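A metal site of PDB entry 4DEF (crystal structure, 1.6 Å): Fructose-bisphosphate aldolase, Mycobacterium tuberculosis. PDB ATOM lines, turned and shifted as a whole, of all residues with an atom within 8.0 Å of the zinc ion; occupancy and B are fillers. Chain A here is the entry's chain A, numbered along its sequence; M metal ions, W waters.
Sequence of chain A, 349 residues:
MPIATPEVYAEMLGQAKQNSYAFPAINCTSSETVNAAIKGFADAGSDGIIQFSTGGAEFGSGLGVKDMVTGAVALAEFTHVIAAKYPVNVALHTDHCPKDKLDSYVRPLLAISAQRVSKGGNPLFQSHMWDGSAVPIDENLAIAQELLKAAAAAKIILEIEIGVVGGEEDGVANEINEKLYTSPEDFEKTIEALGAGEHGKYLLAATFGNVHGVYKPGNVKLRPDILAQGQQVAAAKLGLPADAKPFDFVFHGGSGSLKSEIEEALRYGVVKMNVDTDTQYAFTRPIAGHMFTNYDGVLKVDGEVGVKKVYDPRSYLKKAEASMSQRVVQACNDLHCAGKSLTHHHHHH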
ATOM      1  N   ASN A  27      23.807  32.882  17.164  1.00  0.00           N
ATOM      2  CA  ASN A  27      24.219  31.694  17.906  1.00  0.00           C
ATOM      3  C   ASN A  27      24.530  32.039  19.355  1.00  0.00           C
ATOM      4  O   ASN A  27      25.337  32.923  19.617  1.00  0.00           O
ATOM      5  CB  ASN A  27      25.421  31.026  17.259  1.00  0.00           C
ATOM      6  CG  ASN A  27      25.033  30.199  16.058  1.00  0.00           C
ATOM      7  OD1 ASN A  27      24.847  30.748  14.971  1.00  0.00           O
ATOM      8  ND2 ASN A  27      24.885  28.894  16.242  1.00  0.00           N
ATOM      9  N   GLN A  51      19.614  30.909  18.146  1.00  0.00           N
ATOM     10  CA  GLN A  51      19.859  29.536  17.713  1.00  0.00           C
ATOM     11  C   GLN A  51      20.978  28.848  18.481  1.00  0.00           C
ATOM     12  O   GLN A  51      21.953  29.472  18.890  1.00  0.00           O
ATOM     13  CB  GLN A  51      20.087  29.448  16.200  1.00  0.00           C
ATOM     14  CG  GLN A  51      21.270  30.205  15.632  1.00  0.00           C
ATOM     15  CD  GLN A  51      21.354  30.123  14.114  1.00  0.00           C
ATOM     16  OE1 GLN A  51      20.322  30.034  13.434  1.00  0.00           O
ATOM     17  NE2 GLN A  51      22.565  30.153  13.578  1.00  0.00           N
ATOM     18  N   ASP A  95      20.523  24.911  15.031  1.00  0.00           N
ATOM     19  CA  ASP A  95      21.384  25.105  13.855  1.00  0.00           C
ATOM     20  C   ASP A  95      21.901  23.742  13.346  1.00  0.00           C
ATOM     21  O   ASP A  95      21.633  22.719  13.980  1.00  0.00           O
ATOM     22  CB  ASP A  95      22.535  26.015  14.292  1.00  0.00           C
ATOM     23  CG  ASP A  95      23.241  26.709  13.142  1.00  0.00           C
ATOM     24  OD1 ASP A  95      22.778  26.661  11.983  1.00  0.00           O
ATOM     25  OD2 ASP A  95      24.292  27.328  13.421  1.00  0.00           O
ATOM     26  N   HIS A  96      22.607  23.744  12.206  1.00  0.00           N
ATOM     27  CA  HIS A  96      23.126  22.536  11.490  1.00  0.00           C
ATOM     28  C   HIS A  96      23.085  21.230  12.215  1.00  0.00           C
ATOM     29  O   HIS A  96      23.889  20.980  13.113  1.00  0.00           O
ATOM     30  CB  HIS A  96      24.567  22.739  11.047  1.00  0.00           C
ATOM     31  CG  HIS A  96      24.773  23.931  10.173  1.00  0.00           C
ATOM     32  ND1 HIS A  96      24.786  23.848   8.826  1.00  0.00           N
ATOM     33  CD2 HIS A  96      25.005  25.258  10.491  1.00  0.00           C
ATOM     34  CE1 HIS A  96      24.994  25.068   8.323  1.00  0.00           C
ATOM     35  NE2 HIS A  96      25.133  25.928   9.347  1.00  0.00           N
ATOM     36  N   MET A 129      16.851  23.070  12.197  1.00  0.00           N
ATOM     37  CA  MET A 129      17.564  22.849  10.940  1.00  0.00           C
ATOM     38  C   MET A 129      17.966  21.409  10.705  1.00  0.00           C
ATOM     39  O   MET A 129      18.608  20.784  11.551  1.00  0.00           O
ATOM     40  CB  MET A 129      18.808  23.717  10.813  1.00  0.00           C
ATOM     41  CG  MET A 129      19.441  23.605   9.430  1.00  0.00           C
ATOM     42  SD  MET A 129      21.011  24.446   9.276  1.00  0.00           S
ATOM     43  CE  MET A 129      21.304  24.177   7.527  1.00  0.00           C
ATOM     44  N   ASP A 131      20.421  19.711   8.249  1.00  0.00           N
ATOM     45  CA  ASP A 131      21.498  20.016   7.312  1.00  0.00           C
ATOM     46  C   ASP A 131      21.888  18.764   6.535  1.00  0.00           C
ATOM     47  O   ASP A 131      22.685  17.945   7.019  1.00  0.00           O
ATOM     48  CB  ASP A 131      22.719  20.617   8.022  1.00  0.00           C
ATOM     49  CG  ASP A 131      23.863  20.941   7.075  1.00  0.00           C
ATOM     50  OD1 ASP A 131      23.690  20.832   5.831  1.00  0.00           O
ATOM     51  OD2 ASP A 131      24.939  21.295   7.568  1.00  0.00           O
ATOM     52  N   GLU A 159      14.174  24.221   8.643  1.00  0.00           N
ATOM     53  CA  GLU A 159      15.212  24.792   7.780  1.00  0.00           C
ATOM     54  C   GLU A 159      15.974  23.626   7.172  1.00  0.00           C
ATOM     55  O   GLU A 159      16.324  22.677   7.874  1.00  0.00           O
ATOM     56  CB  GLU A 159      16.186  25.686   8.584  1.00  0.00           C
ATOM     57  CG  GLU A 159      17.262  26.340   7.698  1.00  0.00           C
ATOM     58  CD  GLU A 159      18.182  27.301   8.442  1.00  0.00           C
ATOM     59  OE1 GLU A 159      17.717  28.012   9.345  1.00  0.00           O
ATOM     60  OE2 GLU A 159      19.371  27.395   8.078  1.00  0.00           O
ATOM     61  N   GLU A 161      19.139  22.563   4.024  1.00  0.00           N
ATOM     62  CA  GLU A 161      20.242  23.098   3.241  1.00  0.00           C
ATOM     63  C   GLU A 161      20.550  22.224   2.033  1.00  0.00           C
ATOM     64  O   GLU A 161      20.697  21.007   2.164  1.00  0.00           O
ATOM     65  CB  GLU A 161      21.506  23.248   4.104  1.00  0.00           C
ATOM     66  CG  GLU A 161      22.725  23.661   3.302  1.00  0.00           C
ATOM     67  CD  GLU A 161      23.917  23.981   4.169  1.00  0.00           C
ATOM     68  OE1 GLU A 161      23.754  24.808   5.093  1.00  0.00           O
ATOM     69  OE2 GLU A 161      25.000  23.404   3.936  1.00  0.00           O
ATOM     70  N   VAL A 165      28.123  24.659   2.720  1.00  0.00           N
ATOM     71  CA  VAL A 165      28.764  25.868   3.253  1.00  0.00           C
ATOM     72  C   VAL A 165      30.197  25.537   3.656  1.00  0.00           C
ATOM     73  O   VAL A 165      30.440  24.563   4.376  1.00  0.00           O
ATOM     74  CB  VAL A 165      27.978  26.502   4.439  1.00  0.00           C
ATOM     75  CG1 VAL A 165      28.839  27.459   5.240  1.00  0.00           C
ATOM     76  CG2 VAL A 165      26.765  27.237   3.920  1.00  0.00           C
ATOM     77  N   GLY A 166      31.148  26.346   3.165  1.00  0.00           N
ATOM     78  CA  GLY A 166      32.566  26.159   3.472  1.00  0.00           C
ATOM     79  C   GLY A 166      32.947  26.586   4.878  1.00  0.00           C
ATOM     80  O   GLY A 166      32.114  27.101   5.627  1.00  0.00           O
ATOM     81  N   ALA A 205      18.380  27.087   2.939  1.00  0.00           N
ATOM     82  CA  ALA A 205      19.754  27.541   2.781  1.00  0.00           C
ATOM     83  C   ALA A 205      20.281  26.926   1.492  1.00  0.00           C
ATOM     84  O   ALA A 205      20.462  25.713   1.418  1.00  0.00           O
ATOM     85  CB  ALA A 205      20.592  27.123   3.970  1.00  0.00           C
ATOM     86  N   ASN A 210      29.079  30.927  -0.052  1.00  0.00           N
ATOM     87  CA  ASN A 210      29.064  31.454   1.316  1.00  0.00           C
ATOM     88  C   ASN A 210      29.791  30.564   2.327  1.00  0.00           C
ATOM     89  O   ASN A 210      29.714  29.342   2.260  1.00  0.00           O
ATOM     90  CB  ASN A 210      27.606  31.702   1.753  1.00  0.00           C
ATOM     91  CG  ASN A 210      26.687  30.510   1.461  1.00  0.00           C
ATOM     92  OD1 ASN A 210      26.730  29.905   0.385  1.00  0.00           O
ATOM     93  ND2 ASN A 210      25.853  30.179   2.426  1.00  0.00           N
ATOM     94  N   VAL A 211      30.502  31.188   3.274  1.00  0.00           N
ATOM     95  CA  VAL A 211      31.466  30.480   4.161  1.00  0.00           C
ATOM     96  C   VAL A 211      31.382  30.916   5.644  1.00  0.00           C
ATOM     97  O   VAL A 211      31.197  32.092   5.947  1.00  0.00           O
ATOM     98  CB  VAL A 211      32.914  30.646   3.626  1.00  0.00           C
ATOM     99  CG1 VAL A 211      33.950  30.156   4.630  1.00  0.00           C
ATOM    100  CG2 VAL A 211      33.102  29.922   2.296  1.00  0.00           C
ATOM    101  N   HIS A 212      31.533  29.947   6.554  1.00  0.00           N
ATOM    102  CA  HIS A 212      31.622  30.221   8.000  1.00  0.00           C
ATOM    103  C   HIS A 212      32.946  30.818   8.399  1.00  0.00           C
ATOM    104  O   HIS A 212      34.006  30.309   7.999  1.00  0.00           O
ATOM    105  CB  HIS A 212      31.423  28.951   8.822  1.00  0.00           C
ATOM    106  CG  HIS A 212      29.991  28.492   8.917  1.00  0.00           C
ATOM    107  ND1 HIS A 212      29.624  27.219   8.674  1.00  0.00           N
ATOM    108  CD2 HIS A 212      28.826  29.181   9.244  1.00  0.00           C
ATOM    109  CE1 HIS A 212      28.292  27.105   8.838  1.00  0.00           C
ATOM    110  NE2 HIS A 212      27.807  28.301   9.179  1.00  0.00           N
ATOM    111  N   VAL A 250      17.798  31.366   3.713  1.00  0.00           N
ATOM    112  CA  VAL A 250      18.664  31.598   4.881  1.00  0.00           C
ATOM    113  C   VAL A 250      20.084  31.814   4.393  1.00  0.00           C
ATOM    114  O   VAL A 250      20.583  31.062   3.554  1.00  0.00           O
ATOM    115  CB  VAL A 250      18.646  30.400   5.870  1.00  0.00           C
ATOM    116  CG1 VAL A 250      19.424  30.736   7.143  1.00  0.00           C
ATOM    117  CG2 VAL A 250      17.221  30.039   6.240  1.00  0.00           C
ATOM    118  N   PHE A 251      20.733  32.850   4.927  1.00  0.00           N
ATOM    119  CA  PHE A 251      22.090  33.239   4.541  1.00  0.00           C
ATOM    120  C   PHE A 251      23.056  32.753   5.629  1.00  0.00           C
ATOM    121  O   PHE A 251      23.101  33.310   6.730  1.00  0.00           O
ATOM    122  CB  PHE A 251      22.148  34.768   4.407  1.00  0.00           C
ATOM    123  CG  PHE A 251      23.375  35.318   3.718  1.00  0.00           C
ATOM    124  CD1 PHE A 251      24.614  34.674   3.783  1.00  0.00           C
ATOM    125  CD2 PHE A 251      23.306  36.535   3.043  1.00  0.00           C
ATOM    126  CE1 PHE A 251      25.732  35.211   3.161  1.00  0.00           C
ATOM    127  CE2 PHE A 251      24.422  37.075   2.412  1.00  0.00           C
ATOM    128  CZ  PHE A 251      25.634  36.415   2.466  1.00  0.00           C
ATOM    129  N   HIS A 252      23.796  31.684   5.324  1.00  0.00           N
ATOM    130  CA  HIS A 252      24.815  31.161   6.232  1.00  0.00           C
ATOM    131  C   HIS A 252      26.142  31.804   5.979  1.00  0.00           C
ATOM    132  O   HIS A 252      26.515  32.048   4.825  1.00  0.00           O
ATOM    133  CB  HIS A 252      24.925  29.642   6.130  1.00  0.00           C
ATOM    134  CG  HIS A 252      23.800  28.902   6.810  1.00  0.00           C
ATOM    135  ND1 HIS A 252      23.975  28.180   7.936  1.00  0.00           N
ATOM    136  CD2 HIS A 252      22.458  28.803   6.478  1.00  0.00           C
ATOM    137  CE1 HIS A 252      22.801  27.639   8.297  1.00  0.00           C
ATOM    138  NE2 HIS A 252      21.880  28.009   7.395  1.00  0.00           N
ATOM    139  N   GLY A 253      26.866  32.042   7.066  1.00  0.00           N
ATOM    140  CA  GLY A 253      28.086  32.814   7.051  1.00  0.00           C
ATOM    141  C   GLY A 253      27.791  34.303   6.916  1.00  0.00           C
ATOM    142  O   GLY A 253      28.312  34.951   6.015  1.00  0.00           O
ATOM    143  N   GLY A 254      26.960  34.822   7.808  1.00  0.00           N
ATOM    144  CA  GLY A 254      26.561  36.242   7.762  1.00  0.00           C
ATOM    145  C   GLY A 254      27.644  37.211   8.215  1.00  0.00           C
ATOM    146  O   GLY A 254      27.851  38.253   7.592  1.00  0.00           O
ATOM    147  N   LYS A 272      16.492  35.324   6.860  1.00  0.00           N
ATOM    148  CA  LYS A 272      17.217  34.946   8.071  1.00  0.00           C
ATOM    149  C   LYS A 272      18.706  34.957   7.731  1.00  0.00           C
ATOM    150  O   LYS A 272      19.129  34.308   6.785  1.00  0.00           O
ATOM    151  CB  LYS A 272      16.775  33.545   8.523  1.00  0.00           C
ATOM    152  CG  LYS A 272      17.486  32.942   9.731  1.00  0.00           C
ATOM    153  CD  LYS A 272      16.833  31.604  10.074  1.00  0.00           C
ATOM    154  CE  LYS A 272      17.483  30.850  11.231  1.00  0.00           C
ATOM    155  NZ  LYS A 272      18.763  30.181  10.828  1.00  0.00           N
ATOM    156  N   ASN A 274      22.391  34.158   9.507  1.00  0.00           N
ATOM    157  CA  ASN A 274      23.067  33.600  10.664  1.00  0.00           C
ATOM    158  C   ASN A 274      24.274  34.444  11.063  1.00  0.00           C
ATOM    159  O   ASN A 274      25.080  34.842  10.206  1.00  0.00           O
ATOM    160  CB  ASN A 274      23.479  32.134  10.418  1.00  0.00           C
ATOM    161  CG  ASN A 274      22.285  31.196  10.310  1.00  0.00           C
ATOM    162  OD1 ASN A 274      22.447  29.964  10.310  1.00  0.00           O
ATOM    163  ND2 ASN A 274      21.095  31.748  10.232  1.00  0.00           N
ATOM    164  N   VAL A 275      24.375  34.710  12.360  1.00  0.00           N
ATOM    165  CA  VAL A 275      25.431  35.545  12.958  1.00  0.00           C
ATOM    166  C   VAL A 275      26.067  34.745  14.102  1.00  0.00           C
ATOM    167  O   VAL A 275      25.367  34.263  15.000  1.00  0.00           O
ATOM    168  CB  VAL A 275      24.870  36.908  13.456  1.00  0.00           C
ATOM    169  CG1 VAL A 275      25.929  37.719  14.208  1.00  0.00           C
ATOM    170  CG2 VAL A 275      24.305  37.718  12.298  1.00  0.00           C
ATOM    171  N   ASP A 276      27.390  34.575  14.067  1.00  0.00           N
ATOM    172  CA  ASP A 276      28.055  33.872  15.152  1.00  0.00           C
ATOM    173  C   ASP A 276      29.420  34.485  15.371  1.00  0.00           C
ATOM    174  O   ASP A 276      29.677  35.048  16.432  1.00  0.00           O
ATOM    175  CB  ASP A 276      28.160  32.373  14.850  1.00  0.00           C
ATOM    176  CG  ASP A 276      28.601  31.556  16.048  1.00  0.00           C
ATOM    177  OD1 ASP A 276      28.622  32.075  17.185  1.00  0.00           O
ATOM    178  OD2 ASP A 276      28.899  30.347  15.859  1.00  0.00           O
HETATM  179 ZN    ZN M   1      25.659  27.842   9.192  1.00  0.00          ZN
HETATM  180  O   HOH W   1      25.825  29.874   9.216  1.00  0.00           O
HETATM  181  O   HOH W   2      25.182  28.477  11.209  1.00  0.00           O
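Of the 23 residues printed, 3 come within 4 Å of the zinc ion.
SD of Met 129 is in hydrogen-bond range of N of His 96. A ring nitrogen (ND1) of His 96 is in hydrogen-bond range of the side-chain carboxylate (OD2) of Asp 131, 2.9 Å away. ND1 of His 252 sits close to OD1 of Asn 274, 3.3 Å away. A ring nitrogen (NE2) of His 252 sits at hydrogen-bond distance from the side-chain carboxylate (OE2) of Glu 159 (2.7 Å). The side-chain amide nitrogen (ND2) of Asn 210 sits at hydrogen-bond distance from the backbone carbonyl oxygen (O) of His 252, at 3.1 Å. N of His 212 sits at hydrogen-bond distance from O of Gly 166 (3.0 Å).
The zinc ion is bound by NE2 of His 96, water W1, ND1 of His 252, water W2 and NE2 of His 212. The zinc ion has five donor atoms within binding distance.
Water W2 lies within hydrogen-bond range of OD2 of Asp 95 and OD1 of Asn 274.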
